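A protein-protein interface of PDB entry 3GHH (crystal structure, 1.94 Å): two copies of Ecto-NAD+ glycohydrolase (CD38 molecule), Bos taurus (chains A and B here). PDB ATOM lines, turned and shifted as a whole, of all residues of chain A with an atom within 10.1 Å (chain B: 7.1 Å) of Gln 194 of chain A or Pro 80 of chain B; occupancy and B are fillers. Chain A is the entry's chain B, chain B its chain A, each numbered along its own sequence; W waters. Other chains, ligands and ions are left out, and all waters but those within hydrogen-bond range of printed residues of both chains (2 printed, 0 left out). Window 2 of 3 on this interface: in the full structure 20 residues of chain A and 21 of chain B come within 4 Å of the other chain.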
ATOM      1  N   CYS A  81      17.516 -26.645 -37.111  1.00  0.00           N
ATOM      2  CA  CYS A  81      16.697 -25.723 -36.334  1.00  0.00           C
ATOM      3  C   CYS A  81      16.647 -24.362 -37.011  1.00  0.00           C
ATOM      4  O   CYS A  81      17.644 -23.899 -37.587  1.00  0.00           O
ATOM      5  CB  CYS A  81      17.238 -25.571 -34.907  1.00  0.00           C
ATOM      6  SG  CYS A  81      17.246 -27.096 -33.915  1.00  0.00           S
ATOM      7  N   GLY A  82      15.479 -23.734 -36.944  1.00  0.00           N
ATOM      8  CA  GLY A  82      15.276 -22.399 -37.479  1.00  0.00           C
ATOM      9  C   GLY A  82      15.124 -22.331 -38.985  1.00  0.00           C
ATOM     10  O   GLY A  82      15.027 -21.248 -39.561  1.00  0.00           O
ATOM     11  N   ALA A 161      10.604 -29.473 -35.986  1.00  0.00           N
ATOM     12  CA  ALA A 161      10.917 -28.050 -35.852  1.00  0.00           C
ATOM     13  C   ALA A 161      11.568 -27.734 -34.503  1.00  0.00           C
ATOM     14  O   ALA A 161      11.238 -28.342 -33.489  1.00  0.00           O
ATOM     15  CB  ALA A 161       9.665 -27.204 -36.057  1.00  0.00           C
ATOM     16  N   CYS A 162      12.495 -26.783 -34.502  1.00  0.00           N
ATOM     17  CA  CYS A 162      13.099 -26.315 -33.258  1.00  0.00           C
ATOM     18  C   CYS A 162      13.541 -24.864 -33.393  1.00  0.00           C
ATOM     19  O   CYS A 162      13.669 -24.349 -34.506  1.00  0.00           O
ATOM     20  CB  CYS A 162      14.259 -27.217 -32.820  1.00  0.00           C
ATOM     21  SG  CYS A 162      15.334 -27.750 -34.166  1.00  0.00           S
ATOM     22  N   ASN A 163      13.767 -24.220 -32.248  1.00  0.00           N
ATOM     23  CA  ASN A 163      14.043 -22.788 -32.174  1.00  0.00           C
ATOM     24  C   ASN A 163      12.954 -21.992 -32.886  1.00  0.00           C
ATOM     25  O   ASN A 163      11.773 -22.296 -32.740  1.00  0.00           O
ATOM     26  CB  ASN A 163      15.444 -22.454 -32.702  1.00  0.00           C
ATOM     27  CG  ASN A 163      16.550 -23.112 -31.883  1.00  0.00           C
ATOM     28  OD1 ASN A 163      16.322 -23.532 -30.749  1.00  0.00           O
ATOM     29  ND2 ASN A 163      17.746 -23.215 -32.461  1.00  0.00           N
ATOM     30  N   THR A 164      13.342 -20.984 -33.660  1.00  0.00           N
ATOM     31  CA  THR A 164      12.360 -20.092 -34.264  1.00  0.00           C
ATOM     32  C   THR A 164      11.925 -20.553 -35.650  1.00  0.00           C
ATOM     33  O   THR A 164      12.743 -20.681 -36.561  1.00  0.00           O
ATOM     34  CB  THR A 164      12.888 -18.651 -34.350  1.00  0.00           C
ATOM     35  OG1 THR A 164      13.331 -18.234 -33.053  1.00  0.00           O
ATOM     36  CG2 THR A 164      11.795 -17.713 -34.832  1.00  0.00           C
ATOM     37  N   VAL A 165      10.631 -20.803 -35.807  1.00  0.00           N
ATOM     38  CA  VAL A 165      10.098 -21.218 -37.101  1.00  0.00           C
ATOM     39  C   VAL A 165       8.937 -20.330 -37.547  1.00  0.00           C
ATOM     40  O   VAL A 165       8.349 -19.604 -36.744  1.00  0.00           O
ATOM     41  CB  VAL A 165       9.675 -22.700 -37.093  1.00  0.00           C
ATOM     42  CG1 VAL A 165      10.848 -23.572 -36.672  1.00  0.00           C
ATOM     43  CG2 VAL A 165       8.485 -22.916 -36.174  1.00  0.00           C
ATOM     44  N   ASN A 190       1.523 -30.244 -33.812  1.00  0.00           N
ATOM     45  CA  ASN A 190       2.635 -31.164 -33.580  1.00  0.00           C
ATOM     46  C   ASN A 190       3.987 -30.468 -33.337  1.00  0.00           C
ATOM     47  O   ASN A 190       5.022 -31.121 -33.211  1.00  0.00           O
ATOM     48  CB  ASN A 190       2.717 -32.210 -34.703  1.00  0.00           C
ATOM     49  CG  ASN A 190       1.759 -33.381 -34.481  1.00  0.00           C
ATOM     50  OD1 ASN A 190       0.848 -33.623 -35.278  1.00  0.00           O
ATOM     51  ND2 ASN A 190       1.959 -34.102 -33.384  1.00  0.00           N
ATOM     52  N   LEU A 191       3.962 -29.140 -33.258  1.00  0.00           N
ATOM     53  CA  LEU A 191       5.142 -28.360 -32.888  1.00  0.00           C
ATOM     54  C   LEU A 191       5.572 -28.637 -31.443  1.00  0.00           C
ATOM     55  O   LEU A 191       4.738 -28.706 -30.540  1.00  0.00           O
ATOM     56  CB  LEU A 191       4.858 -26.868 -33.069  1.00  0.00           C
ATOM     57  CG  LEU A 191       4.424 -26.385 -34.455  1.00  0.00           C
ATOM     58  CD1 LEU A 191       3.977 -24.928 -34.404  1.00  0.00           C
ATOM     59  CD2 LEU A 191       5.547 -26.564 -35.480  1.00  0.00           C
ATOM     60  N   ARG A 192       6.874 -28.799 -31.227  1.00  0.00           N
ATOM     61  CA  ARG A 192       7.398 -29.112 -29.898  1.00  0.00           C
ATOM     62  C   ARG A 192       7.325 -27.901 -28.976  1.00  0.00           C
ATOM     63  O   ARG A 192       7.414 -26.763 -29.430  1.00  0.00           O
ATOM     64  CB  ARG A 192       8.852 -29.581 -29.978  1.00  0.00           C
ATOM     65  CG  ARG A 192       9.068 -30.904 -30.699  1.00  0.00           C
ATOM     66  CD  ARG A 192      10.554 -31.118 -30.974  1.00  0.00           C
ATOM     67  NE  ARG A 192      11.314 -31.298 -29.737  1.00  0.00           N
ATOM     68  CZ  ARG A 192      12.641 -31.379 -29.673  1.00  0.00           C
ATOM     69  NH1 ARG A 192      13.378 -31.284 -30.776  1.00  0.00           N
ATOM     70  NH2 ARG A 192      13.232 -31.549 -28.499  1.00  0.00           N
ATOM     71  N   PRO A 193       7.179 -28.147 -27.669  1.00  0.00           N
ATOM     72  CA  PRO A 193       7.174 -27.042 -26.707  1.00  0.00           C
ATOM     73  C   PRO A 193       8.455 -26.232 -26.831  1.00  0.00           C
ATOM     74  O   PRO A 193       9.502 -26.791 -27.167  1.00  0.00           O
ATOM     75  CB  PRO A 193       7.133 -27.755 -25.352  1.00  0.00           C
ATOM     76  CG  PRO A 193       6.578 -29.112 -25.641  1.00  0.00           C
ATOM     77  CD  PRO A 193       7.077 -29.461 -27.012  1.00  0.00           C
ATOM     78  N   GLN A 194       8.359 -24.930 -26.580  1.00  0.00           N
ATOM     79  CA  GLN A 194       9.518 -24.038 -26.556  1.00  0.00           C
ATOM     80  C   GLN A 194      10.000 -23.647 -27.957  1.00  0.00           C
ATOM     81  O   GLN A 194      10.813 -22.726 -28.119  1.00  0.00           O
ATOM     82  CB  GLN A 194      10.635 -24.632 -25.689  1.00  0.00           C
ATOM     83  CG  GLN A 194      10.139 -25.067 -24.301  1.00  0.00           C
ATOM     84  CD  GLN A 194      11.052 -26.083 -23.631  1.00  0.00           C
ATOM     85  OE1 GLN A 194      12.276 -25.959 -23.677  1.00  0.00           O
ATOM     86  NE2 GLN A 194      10.457 -27.094 -23.001  1.00  0.00           N
ATOM     87  N   VAL A 195       9.486 -24.340 -28.970  1.00  0.00           N
ATOM     88  CA  VAL A 195       9.582 -23.846 -30.337  1.00  0.00           C
ATOM     89  C   VAL A 195       8.870 -22.499 -30.373  1.00  0.00           C
ATOM     90  O   VAL A 195       7.813 -22.345 -29.773  1.00  0.00           O
ATOM     91  CB  VAL A 195       8.883 -24.786 -31.336  1.00  0.00           C
ATOM     92  CG1 VAL A 195       8.719 -24.101 -32.687  1.00  0.00           C
ATOM     93  CG2 VAL A 195       9.649 -26.095 -31.475  1.00  0.00           C
ATOM     94  N   GLU A 196       9.453 -21.524 -31.064  1.00  0.00           N
ATOM     95  CA  GLU A 196       8.812 -20.227 -31.248  1.00  0.00           C
ATOM     96  C   GLU A 196       8.282 -20.060 -32.679  1.00  0.00           C
ATOM     97  O   GLU A 196       9.058 -19.959 -33.632  1.00  0.00           O
ATOM     98  CB  GLU A 196       9.791 -19.100 -30.910  1.00  0.00           C
ATOM     99  N   LEU A 197       6.961 -20.016 -32.824  1.00  0.00           N
ATOM    100  CA  LEU A 197       6.339 -19.859 -34.138  1.00  0.00           C
ATOM    101  C   LEU A 197       6.025 -18.406 -34.473  1.00  0.00           C
ATOM    102  O   LEU A 197       5.278 -17.740 -33.754  1.00  0.00           O
ATOM    103  CB  LEU A 197       5.054 -20.681 -34.218  1.00  0.00           C
ATOM    104  CG  LEU A 197       4.259 -20.598 -35.523  1.00  0.00           C
ATOM    105  CD1 LEU A 197       5.108 -21.001 -36.729  1.00  0.00           C
ATOM    106  CD2 LEU A 197       3.010 -21.464 -35.430  1.00  0.00           C
ATOM    107  N   GLU A 198       6.593 -17.920 -35.572  1.00  0.00           N
ATOM    108  CA  GLU A 198       6.247 -16.605 -36.089  1.00  0.00           C
ATOM    109  C   GLU A 198       5.230 -16.752 -37.207  1.00  0.00           C
ATOM    110  O   GLU A 198       5.507 -17.398 -38.216  1.00  0.00           O
ATOM    111  CB  GLU A 198       7.476 -15.896 -36.653  1.00  0.00           C
ATOM    112  CG  GLU A 198       8.571 -15.605 -35.658  1.00  0.00           C
ATOM    113  CD  GLU A 198       9.718 -14.853 -36.298  1.00  0.00           C
ATOM    114  OE1 GLU A 198       9.660 -14.612 -37.525  1.00  0.00           O
ATOM    115  OE2 GLU A 198      10.679 -14.505 -35.580  1.00  0.00           O
ATOM    116  N   LEU A 225      -1.354 -23.346 -29.945  1.00  0.00           N
ATOM    117  CA  LEU A 225       0.027 -23.175 -29.505  1.00  0.00           C
ATOM    118  C   LEU A 225       0.100 -23.131 -27.984  1.00  0.00           C
ATOM    119  O   LEU A 225       0.858 -23.887 -27.370  1.00  0.00           O
ATOM    120  CB  LEU A 225       0.624 -21.909 -30.110  1.00  0.00           C
ATOM    121  CG  LEU A 225       0.481 -21.826 -31.629  1.00  0.00           C
ATOM    122  CD1 LEU A 225       1.254 -20.649 -32.177  1.00  0.00           C
ATOM    123  CD2 LEU A 225       0.941 -23.122 -32.279  1.00  0.00           C
ATOM    124  N   ASP A 226      -0.684 -22.237 -27.382  1.00  0.00           N
ATOM    125  CA  ASP A 226      -0.913 -22.282 -25.944  1.00  0.00           C
ATOM    126  C   ASP A 226      -1.406 -23.691 -25.644  1.00  0.00           C
ATOM    127  O   ASP A 226      -2.174 -24.257 -26.419  1.00  0.00           O
ATOM    128  CB  ASP A 226      -1.988 -21.274 -25.524  1.00  0.00           C
ATOM    129  CG  ASP A 226      -1.589 -19.832 -25.789  1.00  0.00           C
ATOM    130  OD1 ASP A 226      -0.417 -19.584 -26.143  1.00  0.00           O
ATOM    131  OD2 ASP A 226      -2.456 -18.940 -25.634  1.00  0.00           O
ATOM    132  N   GLY A 227      -0.974 -24.271 -24.531  1.00  0.00           N
ATOM    133  CA  GLY A 227      -1.426 -25.607 -24.192  1.00  0.00           C
ATOM    134  C   GLY A 227      -0.607 -26.686 -24.877  1.00  0.00           C
ATOM    135  O   GLY A 227      -0.809 -27.879 -24.638  1.00  0.00           O
ATOM    136  N   ARG A 228       0.312 -26.255 -25.730  1.00  0.00           N
ATOM    137  CA  ARG A 228       1.342 -27.138 -26.225  1.00  0.00           C
ATOM    138  C   ARG A 228       2.678 -26.570 -25.778  1.00  0.00           C
ATOM    139  O   ARG A 228       3.660 -27.234 -25.759  1.00  0.00           O
ATOM    140  CB  ARG A 228       1.262 -27.310 -27.741  1.00  0.00           C
ATOM    141  CG  ARG A 228       0.673 -28.648 -28.160  1.00  0.00           C
ATOM    142  CD  ARG A 228       1.183 -29.104 -29.494  1.00  0.00           C
ATOM    143  NE  ARG A 228       2.425 -29.877 -29.451  1.00  0.00           N
ATOM    144  CZ  ARG A 228       2.525 -31.209 -29.437  1.00  0.00           C
ATOM    145  NH1 ARG A 228       1.461 -31.982 -29.400  1.00  0.00           N
ATOM    146  NH2 ARG A 228       3.721 -31.783 -29.437  1.00  0.00           N
ATOM    147  N   ASN A 229       2.661 -25.315 -25.392  1.00  0.00           N
ATOM    148  CA  ASN A 229       3.830 -24.611 -24.880  1.00  0.00           C
ATOM    149  C   ASN A 229       4.684 -24.034 -25.999  1.00  0.00           C
ATOM    150  O   ASN A 229       5.907 -23.920 -25.877  1.00  0.00           O
ATOM    151  CB  ASN A 229       4.670 -25.514 -23.976  1.00  0.00           C
ATOM    152  CG  ASN A 229       5.083 -24.825 -22.700  1.00  0.00           C
ATOM    153  OD1 ASN A 229       4.274 -24.659 -21.785  1.00  0.00           O
ATOM    154  ND2 ASN A 229       6.347 -24.415 -22.628  1.00  0.00           N
ATOM    155  N   VAL A 230       4.024 -23.673 -27.093  1.00  0.00           N
ATOM    156  CA  VAL A 230       4.697 -23.041 -28.209  1.00  0.00           C
ATOM    157  C   VAL A 230       4.515 -21.537 -28.112  1.00  0.00           C
ATOM    158  O   VAL A 230       3.388 -21.044 -28.064  1.00  0.00           O
ATOM    159  CB  VAL A 230       4.129 -23.532 -29.553  1.00  0.00           C
ATOM    160  CG1 VAL A 230       4.891 -22.906 -30.711  1.00  0.00           C
ATOM    161  CG2 VAL A 230       4.180 -25.050 -29.625  1.00  0.00           C
ATOM    162  N   LYS A 231       5.629 -20.812 -28.078  1.00  0.00           N
ATOM    163  CA  LYS A 231       5.603 -19.354 -28.076  1.00  0.00           C
ATOM    164  C   LYS A 231       5.109 -18.846 -29.430  1.00  0.00           C
ATOM    165  O   LYS A 231       5.301 -19.510 -30.450  1.00  0.00           O
ATOM    166  CB  LYS A 231       7.000 -18.808 -27.773  1.00  0.00           C
ATOM    167  CG  LYS A 231       7.055 -17.309 -27.535  1.00  0.00           C
ATOM    168  CD  LYS A 231       8.451 -16.880 -27.100  1.00  0.00           C
ATOM    169  CE  LYS A 231       8.898 -17.633 -25.850  1.00  0.00           C
ATOM    170  NZ  LYS A 231      10.301 -17.296 -25.465  1.00  0.00           N
ATOM    171  N   PHE A 232       4.484 -17.671 -29.450  1.00  0.00           N
ATOM    172  CA  PHE A 232       3.838 -17.188 -30.670  1.00  0.00           C
ATOM    173  C   PHE A 232       4.025 -15.692 -30.934  1.00  0.00           C
ATOM    174  O   PHE A 232       3.728 -14.860 -30.078  1.00  0.00           O
ATOM    175  CB  PHE A 232       2.345 -17.543 -30.639  1.00  0.00           C
ATOM    176  CG  PHE A 232       1.598 -17.160 -31.892  1.00  0.00           C
ATOM    177  CD1 PHE A 232       2.024 -17.600 -33.132  1.00  0.00           C
ATOM    178  CD2 PHE A 232       0.459 -16.373 -31.823  1.00  0.00           C
ATOM    179  CE1 PHE A 232       1.335 -17.254 -34.284  1.00  0.00           C
ATOM    180  CE2 PHE A 232      -0.236 -16.023 -32.971  1.00  0.00           C
ATOM    181  CZ  PHE A 232       0.205 -16.463 -34.203  1.00  0.00           C
ATOM    182  N   ARG B  36       7.840 -36.008 -16.096  1.00  0.00           N
ATOM    183  CA  ARG B  36       7.663 -34.963 -17.049  1.00  0.00           C
ATOM    184  C   ARG B  36       6.201 -34.618 -17.331  1.00  0.00           C
ATOM    185  O   ARG B  36       5.751 -34.717 -18.438  1.00  0.00           O
ATOM    186  CB  ARG B  36       8.352 -35.309 -18.344  1.00  0.00           C
ATOM    187  CG  ARG B  36       9.808 -35.118 -18.367  1.00  0.00           C
ATOM    188  CD  ARG B  36      10.225 -34.825 -19.791  1.00  0.00           C
ATOM    189  NE  ARG B  36      10.172 -33.409 -20.136  1.00  0.00           N
ATOM    190  CZ  ARG B  36      10.346 -32.919 -21.363  1.00  0.00           C
ATOM    191  NH1 ARG B  36      10.561 -33.709 -22.395  1.00  0.00           N
ATOM    192  NH2 ARG B  36      10.296 -31.625 -21.558  1.00  0.00           N
ATOM    193  N   THR B  78      12.138 -36.962 -27.850  1.00  0.00           N
ATOM    194  CA  THR B  78      12.604 -35.592 -28.009  1.00  0.00           C
ATOM    195  C   THR B  78      12.940 -34.989 -26.647  1.00  0.00           C
ATOM    196  O   THR B  78      12.240 -35.218 -25.664  1.00  0.00           O
ATOM    197  CB  THR B  78      11.546 -34.728 -28.718  1.00  0.00           C
ATOM    198  OG1 THR B  78      10.442 -34.502 -27.831  1.00  0.00           O
ATOM    199  CG2 THR B  78      11.037 -35.445 -29.965  1.00  0.00           C
ATOM    200  N   VAL B  79      14.022 -34.225 -26.604  1.00  0.00           N
ATOM    201  CA  VAL B  79      14.549 -33.660 -25.373  1.00  0.00           C
ATOM    202  C   VAL B  79      14.725 -32.171 -25.635  1.00  0.00           C
ATOM    203  O   VAL B  79      15.120 -31.789 -26.737  1.00  0.00           O
ATOM    204  CB  VAL B  79      15.904 -34.315 -25.020  1.00  0.00           C
ATOM    205  CG1 VAL B  79      16.636 -33.537 -23.930  1.00  0.00           C
ATOM    206  CG2 VAL B  79      15.696 -35.764 -24.602  1.00  0.00           C
ATOM    207  N   PRO B  80      14.405 -31.320 -24.644  1.00  0.00           N
ATOM    208  CA  PRO B  80      14.526 -29.876 -24.875  1.00  0.00           C
ATOM    209  C   PRO B  80      15.937 -29.483 -25.325  1.00  0.00           C
ATOM    210  O   PRO B  80      16.924 -30.092 -24.910  1.00  0.00           O
ATOM    211  CB  PRO B  80      14.214 -29.270 -23.503  1.00  0.00           C
ATOM    212  CG  PRO B  80      13.364 -30.298 -22.823  1.00  0.00           C
ATOM    213  CD  PRO B  80      13.872 -31.629 -23.306  1.00  0.00           C
ATOM    214  N   CYS B  81      16.015 -28.473 -26.177  1.00  0.00           N
ATOM    215  CA  CYS B  81      17.291 -28.002 -26.703  1.00  0.00           C
ATOM    216  C   CYS B  81      18.286 -27.664 -25.589  1.00  0.00           C
ATOM    217  O   CYS B  81      17.951 -26.978 -24.621  1.00  0.00           O
ATOM    218  CB  CYS B  81      17.055 -26.793 -27.601  1.00  0.00           C
ATOM    219  SG  CYS B  81      15.843 -27.085 -28.914  1.00  0.00           S
ATOM    220  N   GLY B  82      19.507 -28.170 -25.723  1.00  0.00           N
ATOM    221  CA  GLY B  82      20.548 -27.921 -24.742  1.00  0.00           C
ATOM    222  C   GLY B  82      20.544 -28.809 -23.507  1.00  0.00           C
ATOM    223  O   GLY B  82      21.365 -28.623 -22.612  1.00  0.00           O
ATOM    224  N   GLN B  83      19.629 -29.772 -23.450  1.00  0.00           N
ATOM    225  CA  GLN B  83      19.572 -30.698 -22.328  1.00  0.00           C
ATOM    226  C   GLN B  83      19.946 -32.125 -22.708  1.00  0.00           C
ATOM    227  O   GLN B  83      19.944 -33.006 -21.859  1.00  0.00           O
ATOM    228  CB  GLN B  83      18.162 -30.735 -21.738  1.00  0.00           C
ATOM    229  CG  GLN B  83      17.873 -29.659 -20.734  1.00  0.00           C
ATOM    230  CD  GLN B  83      16.598 -29.938 -19.971  1.00  0.00           C
ATOM    231  OE1 GLN B  83      15.656 -29.152 -20.014  1.00  0.00           O
ATOM    232  NE2 GLN B  83      16.556 -31.072 -19.276  1.00  0.00           N
ATOM    233  N   GLN B  84      20.247 -32.360 -23.981  1.00  0.00           N
ATOM    234  CA  GLN B  84      20.411 -33.730 -24.460  1.00  0.00           C
ATOM    235  C   GLN B  84      21.801 -34.297 -24.195  1.00  0.00           C
ATOM    236  O   GLN B  84      22.814 -33.624 -24.417  1.00  0.00           O
ATOM    237  CB  GLN B  84      20.084 -33.810 -25.948  1.00  0.00           C
ATOM    238  CG  GLN B  84      19.964 -35.221 -26.483  1.00  0.00           C
ATOM    239  CD  GLN B  84      19.048 -35.302 -27.687  1.00  0.00           C
ATOM    240  OE1 GLN B  84      18.321 -34.360 -27.980  1.00  0.00           O
ATOM    241  NE2 GLN B  84      19.081 -36.432 -28.393  1.00  0.00           N
ATOM    242  N   MET B 104      19.078 -34.942 -19.836  1.00  0.00           N
ATOM    243  CA  MET B 104      18.338 -36.124 -20.243  1.00  0.00           C
ATOM    244  C   MET B 104      19.103 -36.997 -21.223  1.00  0.00           C
ATOM    245  O   MET B 104      19.499 -36.544 -22.288  1.00  0.00           O
ATOM    246  CB  MET B 104      16.997 -35.726 -20.859  1.00  0.00           C
ATOM    247  CG  MET B 104      16.003 -35.145 -19.854  1.00  0.00           C
ATOM    248  SD  MET B 104      14.462 -34.621 -20.641  1.00  0.00           S
ATOM    249  CE  MET B 104      13.751 -36.202 -21.037  1.00  0.00           C
ATOM    250  N   SER B 160      16.441 -35.548 -33.484  1.00  0.00           N
ATOM    251  CA  SER B 160      15.662 -34.475 -32.881  1.00  0.00           C
ATOM    252  C   SER B 160      16.545 -33.558 -32.024  1.00  0.00           C
ATOM    253  O   SER B 160      16.086 -32.531 -31.540  1.00  0.00           O
ATOM    254  CB  SER B 160      14.520 -35.065 -32.049  1.00  0.00           C
ATOM    255  OG  SER B 160      15.050 -35.889 -31.037  1.00  0.00           O
ATOM    256  N   ALA B 161      17.812 -33.933 -31.854  1.00  0.00           N
ATOM    257  CA  ALA B 161      18.757 -33.166 -31.042  1.00  0.00           C
ATOM    258  C   ALA B 161      18.802 -31.715 -31.499  1.00  0.00           C
ATOM    259  O   ALA B 161      18.673 -31.431 -32.685  1.00  0.00           O
ATOM    260  CB  ALA B 161      20.148 -33.785 -31.126  1.00  0.00           C
ATOM    261  N   CYS B 162      18.968 -30.787 -30.565  1.00  0.00           N
ATOM    262  CA  CYS B 162      18.981 -29.379 -30.954  1.00  0.00           C
ATOM    263  C   CYS B 162      19.864 -28.509 -30.059  1.00  0.00           C
ATOM    264  O   CYS B 162      19.965 -28.732 -28.844  1.00  0.00           O
ATOM    265  CB  CYS B 162      17.552 -28.816 -31.064  1.00  0.00           C
ATOM    266  SG  CYS B 162      16.554 -28.888 -29.555  1.00  0.00           S
ATOM    267  N   ASN B 163      20.487 -27.516 -30.682  1.00  0.00           N
ATOM    268  CA  ASN B 163      21.436 -26.633 -30.014  1.00  0.00           C
ATOM    269  C   ASN B 163      22.645 -27.399 -29.461  1.00  0.00           C
ATOM    270  O   ASN B 163      23.210 -28.245 -30.155  1.00  0.00           O
ATOM    271  CB  ASN B 163      20.725 -25.782 -28.966  1.00  0.00           C
ATOM    272  CG  ASN B 163      19.743 -24.797 -29.600  1.00  0.00           C
ATOM    273  OD1 ASN B 163      19.888 -24.430 -30.771  1.00  0.00           O
ATOM    274  ND2 ASN B 163      18.754 -24.365 -28.834  1.00  0.00           N
ATOM    275  N   THR B 164      23.050 -27.122 -28.230  1.00  0.00           N
ATOM    276  CA  THR B 164      24.223 -27.810 -27.689  1.00  0.00           C
ATOM    277  C   THR B 164      23.839 -29.189 -27.160  1.00  0.00           C
ATOM    278  O   THR B 164      22.888 -29.332 -26.394  1.00  0.00           O
ATOM    279  CB  THR B 164      24.918 -26.993 -26.585  1.00  0.00           C
ATOM    280  OG1 THR B 164      25.245 -25.696 -27.090  1.00  0.00           O
ATOM    281  CG2 THR B 164      26.218 -27.685 -26.130  1.00  0.00           C
HETATM  282  O   HOH W   1      15.325 -25.736 -23.941  1.00  0.00           O
HETATM  283  O   HOH W   2      20.570 -26.627 -33.361  1.00  0.00           O
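The guanidinium group of Arg 192 of chain A is in hydrogen-bond range of the backbone carbonyl oxygen of Val 79 of chain B. The backbone carbonyl oxygen (O) of Ser 160 of chain B lies within hydrogen-bond range of the guanidinium group (NH1) of Arg 192 of chain A (3.1 Å). The side-chain amide oxygen (OD1) of Asn 163 of chain B sits at hydrogen-bond distance from the side-chain amide nitrogen (ND2) of Asn 163 of chain A (3.0 Å).
SG of Cys 81 of chain B is disulfide-bonded to SG of Cys 162 of chain B (2.0 Å). The backbone carbonyl oxygen (O) of Cys 162 of chain B lies within hydrogen-bond range of the backbone NH (N) of Gly 82 of chain B, at 3.2 Å. SG of Cys 81 of chain A forms a disulfide with SG of Cys 162 of chain A (2.0 Å). The backbone NH (N) of Gly 82 of chain A sits at hydrogen-bond distance from the backbone carbonyl oxygen (O) of Cys 162 of chain A. The backbone carbonyl oxygen of Asn 163 of chain A is in hydrogen-bond range of the backbone NH of Glu 196 of chain A, at 3.0 Å. The backbone carbonyl oxygen of Asn 229 of chain A lies within hydrogen-bond range of the backbone NH of Gln 194 of chain A.
Cys 81 of chain A touches Cys 162 of chain B (SG to CB, 3.3 Å). CB of Cys 162 of chain B touches SG of Cys 162 of chain A (3.96 Å). Thr 78 of chain B touches Arg 192 of chain A. Pro 80 of chain B touches Gln 194 of chain A.
Printed residues of chain B within 4 Å of Asn 163 of chain A: Asn 163 (3.0 Å). Printed residues of chain B within 4 Å of Arg 192 of chain A: Thr 78 (3.6 Å), Val 79 (2.6 Å) and Ser 160 (3.1 Å). Of chain B, only Pro 80 comes within 4 Å of Gln 194 of chain A. Val 79 of chain B touches just one residue of chain A: Arg 192. Of the printed residues of chain A, Pro 80 of chain B touches Gln 194. Cys 81 of chain B touches none of the printed residues of chain A. No residue of chain A comes within 4 Å of Gly 82 of chain B. Of the printed residues of chain A, Ser 160 of chain B touches Arg 192 (3.1 Å). Of the printed residues of chain A, Asn 163 of chain B touches Asn 163. The nearest residue of chain A that does not touch Pro 80 of chain B is Arg 192 of chain A (4.04 Å). The nearest printed residue of chain B that does not touch Arg 192 of chain A is Pro 80 of chain B (4.04 Å).
Of the 14 printed residues of chain B, 6 touch a printed residue of chain A. Of the 24 printed residues of chain A, 5 touch a printed residue of chain B. Printed residues of chain A that touch a printed residue of chain B: Cys 81, Cys 162, Asn 163, Arg 192 and Gln 194. Among the printed residues, no Asp or Glu carboxylate lies within 4 Å of a Lys or Arg side-chain nitrogen of the other chain.
Cys 81 of chain A touches Cys 162 of chain B, but with the chains exchanged Cys 162 of chain A does not touch Cys 81 of chain B (4.2 Å). Cys 162 of chain A touches its own counterpart, Cys 162 of chain B. Asn 163 of chain A touches its own counterpart, Asn 163 of chain B. Positions printed for both chains: 81, 82, 161, 162, 163 and 164. Of the 7 pairs that touch across the chains among the printed residues, 2 have their exchanged pair printed and touching as well.
Water W2 bridges the backbone NH (N) of Asn 163 of chain B (2.8 Å) and the side-chain sulfur (SG) of Cys 81 of chain A (3.4 Å). Water W1 lies within hydrogen-bond range of the backbone carbonyl oxygen (O) of Cys 81 of chain B (3.0 Å) and the side-chain amide oxygen (OE1) of Gln 194 of chain A (3.1 Å).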
